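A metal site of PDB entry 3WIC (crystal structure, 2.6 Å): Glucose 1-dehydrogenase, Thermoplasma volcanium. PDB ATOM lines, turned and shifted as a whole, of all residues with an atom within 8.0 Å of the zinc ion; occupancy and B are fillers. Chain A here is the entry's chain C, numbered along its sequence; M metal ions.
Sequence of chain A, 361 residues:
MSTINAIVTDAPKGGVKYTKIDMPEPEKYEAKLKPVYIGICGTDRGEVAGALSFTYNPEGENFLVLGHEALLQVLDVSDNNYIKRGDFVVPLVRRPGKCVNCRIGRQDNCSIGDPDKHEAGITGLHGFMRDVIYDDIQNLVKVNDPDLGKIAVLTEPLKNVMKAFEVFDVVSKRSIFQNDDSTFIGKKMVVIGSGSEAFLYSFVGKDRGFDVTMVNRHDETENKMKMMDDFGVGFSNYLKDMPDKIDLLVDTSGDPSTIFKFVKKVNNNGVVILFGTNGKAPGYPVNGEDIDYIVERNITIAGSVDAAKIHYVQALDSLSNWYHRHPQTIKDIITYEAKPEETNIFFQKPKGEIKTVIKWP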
ATOM      1  N   ARG A  94      27.919  15.909  21.986  1.00  0.00           N
ATOM      2  CA  ARG A  94      27.072  15.004  22.720  1.00  0.00           C
ATOM      3  C   ARG A  94      26.829  13.808  21.860  1.00  0.00           C
ATOM      4  O   ARG A  94      26.515  13.964  20.693  1.00  0.00           O
ATOM      5  CB  ARG A  94      25.741  15.642  23.064  1.00  0.00           C
ATOM      6  CG  ARG A  94      24.791  14.716  23.804  1.00  0.00           C
ATOM      7  CD  ARG A  94      23.451  15.422  24.035  1.00  0.00           C
ATOM      8  NE  ARG A  94      23.484  16.469  25.072  1.00  0.00           N
ATOM      9  CZ  ARG A  94      22.429  16.838  25.790  1.00  0.00           C
ATOM     10  NH1 ARG A  94      21.247  16.281  25.573  1.00  0.00           N
ATOM     11  NH2 ARG A  94      22.563  17.787  26.716  1.00  0.00           N
ATOM     12  N   ARG A  95      26.994  12.631  22.458  1.00  0.00           N
ATOM     13  CA  ARG A  95      26.785  11.374  21.778  1.00  0.00           C
ATOM     14  C   ARG A  95      25.670  10.614  22.393  1.00  0.00           C
ATOM     15  O   ARG A  95      25.480  10.658  23.628  1.00  0.00           O
ATOM     16  CB  ARG A  95      28.052  10.547  21.775  1.00  0.00           C
ATOM     17  CG  ARG A  95      28.960  10.973  20.628  1.00  0.00           C
ATOM     18  CD  ARG A  95      30.011  11.894  21.131  1.00  0.00           C
ATOM     19  NE  ARG A  95      30.661  12.686  20.112  1.00  0.00           N
ATOM     20  CZ  ARG A  95      31.610  12.265  19.274  1.00  0.00           C
ATOM     21  NH1 ARG A  95      31.972  10.996  19.187  1.00  0.00           N
ATOM     22  NH2 ARG A  95      32.168  13.114  18.463  1.00  0.00           N
ATOM     23  N   PRO A  96      24.904   9.922  21.534  1.00  0.00           N
ATOM     24  CA  PRO A  96      23.666   9.388  22.073  1.00  0.00           C
ATOM     25  C   PRO A  96      23.775   8.083  22.867  1.00  0.00           C
ATOM     26  O   PRO A  96      24.737   7.340  22.731  1.00  0.00           O
ATOM     27  CB  PRO A  96      22.868   9.114  20.806  1.00  0.00           C
ATOM     28  CG  PRO A  96      23.932   8.608  19.852  1.00  0.00           C
ATOM     29  CD  PRO A  96      25.023   9.638  20.093  1.00  0.00           C
ATOM     30  N   GLY A  97      22.738   7.842  23.695  1.00  0.00           N
ATOM     31  CA  GLY A  97      22.438   6.528  24.284  1.00  0.00           C
ATOM     32  C   GLY A  97      21.361   5.763  23.515  1.00  0.00           C
ATOM     33  O   GLY A  97      21.412   5.609  22.257  1.00  0.00           O
ATOM     34  N   LYS A  98      20.373   5.288  24.266  1.00  0.00           N
ATOM     35  CA  LYS A  98      19.323   4.450  23.734  1.00  0.00           C
ATOM     36  C   LYS A  98      17.932   5.020  23.967  1.00  0.00           C
ATOM     37  O   LYS A  98      16.938   4.333  23.720  1.00  0.00           O
ATOM     38  CB  LYS A  98      19.386   3.057  24.352  1.00  0.00           C
ATOM     39  CG  LYS A  98      20.702   2.690  25.040  1.00  0.00           C
ATOM     40  CD  LYS A  98      21.148   1.296  24.659  1.00  0.00           C
ATOM     41  CE  LYS A  98      22.545   0.957  25.150  1.00  0.00           C
ATOM     42  NZ  LYS A  98      23.009  -0.293  24.488  1.00  0.00           N
ATOM     43  N   CYS A  99      17.801   6.261  24.436  1.00  0.00           N
ATOM     44  CA  CYS A  99      16.415   6.749  24.623  1.00  0.00           C
ATOM     45  C   CYS A  99      15.720   7.040  23.245  1.00  0.00           C
ATOM     46  O   CYS A  99      16.330   6.994  22.184  1.00  0.00           O
ATOM     47  CB  CYS A  99      16.358   7.928  25.577  1.00  0.00           C
ATOM     48  SG  CYS A  99      16.664   9.472  24.747  1.00  0.00           S
ATOM     49  N   VAL A 100      14.423   7.285  23.273  1.00  0.00           N
ATOM     50  CA  VAL A 100      13.669   7.413  22.018  1.00  0.00           C
ATOM     51  C   VAL A 100      14.162   8.595  21.180  1.00  0.00           C
ATOM     52  O   VAL A 100      13.878   8.654  19.995  1.00  0.00           O
ATOM     53  CB  VAL A 100      12.149   7.559  22.286  1.00  0.00           C
ATOM     54  CG1 VAL A 100      11.830   8.843  22.996  1.00  0.00           C
ATOM     55  CG2 VAL A 100      11.358   7.476  20.983  1.00  0.00           C
ATOM     56  N   ASN A 101      14.868   9.546  21.798  1.00  0.00           N
ATOM     57  CA  ASN A 101      15.368  10.687  21.088  1.00  0.00           C
ATOM     58  C   ASN A 101      16.807  10.489  20.665  1.00  0.00           C
ATOM     59  O   ASN A 101      17.223  10.900  19.582  1.00  0.00           O
ATOM     60  CB  ASN A 101      15.235  11.916  21.965  1.00  0.00           C
ATOM     61  CG  ASN A 101      13.824  12.517  21.933  1.00  0.00           C
ATOM     62  OD1 ASN A 101      13.327  12.905  20.875  1.00  0.00           O
ATOM     63  ND2 ASN A 101      13.185  12.581  23.085  1.00  0.00           N
ATOM     64  N   CYS A 102      17.566   9.864  21.532  1.00  0.00           N
ATOM     65  CA  CYS A 102      18.927   9.542  21.226  1.00  0.00           C
ATOM     66  C   CYS A 102      19.064   8.653  19.968  1.00  0.00           C
ATOM     67  O   CYS A 102      19.887   8.924  19.113  1.00  0.00           O
ATOM     68  CB  CYS A 102      19.599   8.877  22.444  1.00  0.00           C
ATOM     69  SG  CYS A 102      20.195  10.056  23.700  1.00  0.00           S
ATOM     70  N   ARG A 103      18.236   7.616  19.879  1.00  0.00           N
ATOM     71  CA  ARG A 103      18.331   6.612  18.840  1.00  0.00           C
ATOM     72  C   ARG A 103      17.956   7.138  17.449  1.00  0.00           C
ATOM     73  O   ARG A 103      18.111   6.402  16.454  1.00  0.00           O
ATOM     74  CB  ARG A 103      17.453   5.384  19.179  1.00  0.00           C
ATOM     75  CG  ARG A 103      15.942   5.647  19.003  1.00  0.00           C
ATOM     76  CD  ARG A 103      15.114   4.505  19.555  1.00  0.00           C
ATOM     77  NE  ARG A 103      15.177   4.397  21.019  1.00  0.00           N
ATOM     78  CZ  ARG A 103      14.481   3.537  21.745  1.00  0.00           C
ATOM     79  NH1 ARG A 103      13.664   2.663  21.177  1.00  0.00           N
ATOM     80  NH2 ARG A 103      14.571   3.553  23.037  1.00  0.00           N
ATOM     81  N   ARG A 106      18.756  12.776  17.962  1.00  0.00           N
ATOM     82  CA  ARG A 106      18.358  13.940  18.736  1.00  0.00           C
ATOM     83  C   ARG A 106      18.762  13.762  20.224  1.00  0.00           C
ATOM     84  O   ARG A 106      18.002  14.033  21.148  1.00  0.00           O
ATOM     85  CB  ARG A 106      16.832  14.166  18.610  1.00  0.00           C
ATOM     86  CG  ARG A 106      16.331  14.386  17.170  1.00  0.00           C
ATOM     87  CD  ARG A 106      16.979  15.599  16.498  1.00  0.00           C
ATOM     88  NE  ARG A 106      17.028  16.808  17.376  1.00  0.00           N
ATOM     89  CZ  ARG A 106      16.568  18.013  17.062  1.00  0.00           C
ATOM     90  NH1 ARG A 106      16.022  18.258  15.872  1.00  0.00           N
ATOM     91  NH2 ARG A 106      16.678  19.002  17.916  1.00  0.00           N
ATOM     92  N   GLN A 107      19.989  13.316  20.437  1.00  0.00           N
ATOM     93  CA  GLN A 107      20.517  13.188  21.802  1.00  0.00           C
ATOM     94  C   GLN A 107      20.503  14.549  22.573  1.00  0.00           C
ATOM     95  O   GLN A 107      20.430  14.580  23.800  1.00  0.00           O
ATOM     96  CB  GLN A 107      21.933  12.579  21.768  1.00  0.00           C
ATOM     97  CG  GLN A 107      22.935  13.258  20.841  1.00  0.00           C
ATOM     98  CD  GLN A 107      23.030  12.639  19.432  1.00  0.00           C
ATOM     99  OE1 GLN A 107      22.012  12.215  18.845  1.00  0.00           O
ATOM    100  NE2 GLN A 107      24.264  12.601  18.872  1.00  0.00           N
ATOM    101  N   ASP A 108      20.532  15.650  21.838  1.00  0.00           N
ATOM    102  CA  ASP A 108      20.305  16.992  22.400  1.00  0.00           C
ATOM    103  C   ASP A 108      19.015  17.138  23.192  1.00  0.00           C
ATOM    104  O   ASP A 108      18.924  18.039  24.047  1.00  0.00           O
ATOM    105  CB  ASP A 108      20.351  18.054  21.290  1.00  0.00           C
ATOM    106  CG  ASP A 108      19.204  17.910  20.278  1.00  0.00           C
ATOM    107  OD1 ASP A 108      19.044  16.801  19.645  1.00  0.00           O
ATOM    108  OD2 ASP A 108      18.507  18.952  20.112  1.00  0.00           O
ATOM    109  N   ASN A 109      18.040  16.257  22.871  1.00  0.00           N
ATOM    110  CA  ASN A 109      16.719  16.180  23.518  1.00  0.00           C
ATOM    111  C   ASN A 109      16.485  14.832  24.132  1.00  0.00           C
ATOM    112  O   ASN A 109      15.383  14.248  24.017  1.00  0.00           O
ATOM    113  CB  ASN A 109      15.574  16.411  22.528  1.00  0.00           C
ATOM    114  CG  ASN A 109      15.535  17.795  22.012  1.00  0.00           C
ATOM    115  OD1 ASN A 109      15.888  18.757  22.714  1.00  0.00           O
ATOM    116  ND2 ASN A 109      15.077  17.933  20.763  1.00  0.00           N
ATOM    117  N   CYS A 110      17.532  14.345  24.793  1.00  0.00           N
ATOM    118  CA  CYS A 110      17.502  13.103  25.512  1.00  0.00           C
ATOM    119  C   CYS A 110      16.446  13.126  26.635  1.00  0.00           C
ATOM    120  O   CYS A 110      16.376  14.087  27.402  1.00  0.00           O
ATOM    121  CB  CYS A 110      18.888  12.808  26.091  1.00  0.00           C
ATOM    122  SG  CYS A 110      19.130  11.050  26.494  1.00  0.00           S
ATOM    123  N   SER A 111      15.645  12.058  26.705  1.00  0.00           N
ATOM    124  CA  SER A 111      14.534  11.935  27.616  1.00  0.00           C
ATOM    125  C   SER A 111      14.960  11.462  29.004  1.00  0.00           C
ATOM    126  O   SER A 111      14.192  11.534  29.974  1.00  0.00           O
ATOM    127  CB  SER A 111      13.559  10.927  27.059  1.00  0.00           C
ATOM    128  OG  SER A 111      13.356  11.125  25.662  1.00  0.00           O
ATOM    129  N   ILE A 112      16.174  10.939  29.076  1.00  0.00           N
ATOM    130  CA  ILE A 112      16.721  10.417  30.277  1.00  0.00           C
ATOM    131  C   ILE A 112      17.732  11.357  30.881  1.00  0.00           C
ATOM    132  O   ILE A 112      17.608  11.700  32.017  1.00  0.00           O
ATOM    133  CB  ILE A 112      17.363   9.056  30.000  1.00  0.00           C
ATOM    134  CG1 ILE A 112      16.252   8.074  29.617  1.00  0.00           C
ATOM    135  CG2 ILE A 112      18.167   8.589  31.234  1.00  0.00           C
ATOM    136  CD1 ILE A 112      16.710   6.672  29.251  1.00  0.00           C
ATOM    137  N   GLY A 113      18.724  11.788  30.119  1.00  0.00           N
ATOM    138  CA  GLY A 113      19.825  12.594  30.647  1.00  0.00           C
ATOM    139  C   GLY A 113      21.021  11.717  30.949  1.00  0.00           C
ATOM    140  O   GLY A 113      21.106  10.576  30.472  1.00  0.00           O
ATOM    141  N   ASP A 114      21.947  12.244  31.740  1.00  0.00           N
ATOM    142  CA  ASP A 114      23.013  11.432  32.301  1.00  0.00           C
ATOM    143  C   ASP A 114      22.412  10.253  33.021  1.00  0.00           C
ATOM    144  O   ASP A 114      21.561  10.432  33.877  1.00  0.00           O
ATOM    145  CB  ASP A 114      23.864  12.267  33.216  1.00  0.00           C
ATOM    146  CG  ASP A 114      24.639  13.340  32.447  1.00  0.00           C
ATOM    147  OD1 ASP A 114      25.337  12.965  31.467  1.00  0.00           O
ATOM    148  OD2 ASP A 114      24.547  14.542  32.805  1.00  0.00           O
ATOM    149  N   PRO A 115      22.795   9.027  32.625  1.00  0.00           N
ATOM    150  CA  PRO A 115      23.802   8.810  31.587  1.00  0.00           C
ATOM    151  C   PRO A 115      23.323   8.219  30.263  1.00  0.00           C
ATOM    152  O   PRO A 115      24.009   7.337  29.770  1.00  0.00           O
ATOM    153  CB  PRO A 115      24.750   7.824  32.303  1.00  0.00           C
ATOM    154  CG  PRO A 115      23.808   6.977  33.147  1.00  0.00           C
ATOM    155  CD  PRO A 115      22.523   7.775  33.365  1.00  0.00           C
ATOM    156  N   ASP A 116      22.202   8.635  29.645  1.00  0.00           N
ATOM    157  CA  ASP A 116      21.868   8.030  28.345  1.00  0.00           C
ATOM    158  C   ASP A 116      22.950   8.572  27.406  1.00  0.00           C
ATOM    159  O   ASP A 116      23.627   7.825  26.677  1.00  0.00           O
ATOM    160  CB  ASP A 116      20.446   8.342  27.904  1.00  0.00           C
ATOM    161  CG  ASP A 116      19.952   7.370  26.923  1.00  0.00           C
ATOM    162  OD1 ASP A 116      20.123   6.192  27.161  1.00  0.00           O
ATOM    163  OD2 ASP A 116      19.422   7.814  25.865  1.00  0.00           O
ATOM    164  N   LYS A 117      23.207   9.881  27.575  1.00  0.00           N
ATOM    165  CA  LYS A 117      24.015  10.657  26.667  1.00  0.00           C
ATOM    166  C   LYS A 117      25.313  11.037  27.344  1.00  0.00           C
ATOM    167  O   LYS A 117      25.424  11.067  28.583  1.00  0.00           O
ATOM    168  CB  LYS A 117      23.272  11.939  26.224  1.00  0.00           C
ATOM    169  CG  LYS A 117      22.729  12.817  27.345  1.00  0.00           C
ATOM    170  CD  LYS A 117      23.794  13.656  27.978  1.00  0.00           C
ATOM    171  CE  LYS A 117      23.163  14.654  28.938  1.00  0.00           C
ATOM    172  NZ  LYS A 117      24.130  15.287  29.833  1.00  0.00           N
ATOM    173  N   HIS A 118      26.285  11.334  26.502  1.00  0.00           N
ATOM    174  CA  HIS A 118      27.559  11.801  26.975  1.00  0.00           C
ATOM    175  C   HIS A 118      28.097  12.918  26.121  1.00  0.00           C
ATOM    176  O   HIS A 118      27.973  12.886  24.878  1.00  0.00           O
ATOM    177  CB  HIS A 118      28.541  10.638  26.973  1.00  0.00           C
ATOM    178  CG  HIS A 118      28.132   9.522  27.873  1.00  0.00           C
ATOM    179  ND1 HIS A 118      27.291   8.507  27.452  1.00  0.00           N
ATOM    180  CD2 HIS A 118      28.420   9.288  29.177  1.00  0.00           C
ATOM    181  CE1 HIS A 118      27.067   7.697  28.476  1.00  0.00           C
ATOM    182  NE2 HIS A 118      27.732   8.149  29.525  1.00  0.00           N
HETATM  183 ZN    ZN M   1      18.862   9.487  25.481  1.00  0.00          ZN
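The nearest printed residue that does not touch the zinc ion is Ser 111 (4.3 Å).
O of Asp 116 sits close to N of Gly 97. N of Lys 98 lies within hydrogen-bond range of OD1 of Asp 116. SG of Cys 110 lies close to N of Gly 113, 3.7 Å away. The backbone NH (N) of Gly 97 sits close to the side-chain sulfur (SG) of Cys 102 (3.4 Å). The side-chain sulfur (SG) of Cys 99 sits close to the backbone NH (N) of Ser 111, at 3.4 Å. The side-chain sulfur of Cys 99 sits close to the backbone NH of Asn 101. The guanidinium group of Arg 103 is in hydrogen-bond range of the backbone carbonyl oxygen of Cys 99 (3.1 Å).
OD2 of Asp 116 is bound to the zinc ion, at 1.8 Å. The zinc ion is bound by SG of Cys 110. The side-chain sulfur (SG) of Cys 102 is bound to the zinc ion, 2.3 Å away. SG of Cys 99 is bound to the zinc ion (2.3 Å). The zinc ion has four donor atoms within binding distance.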
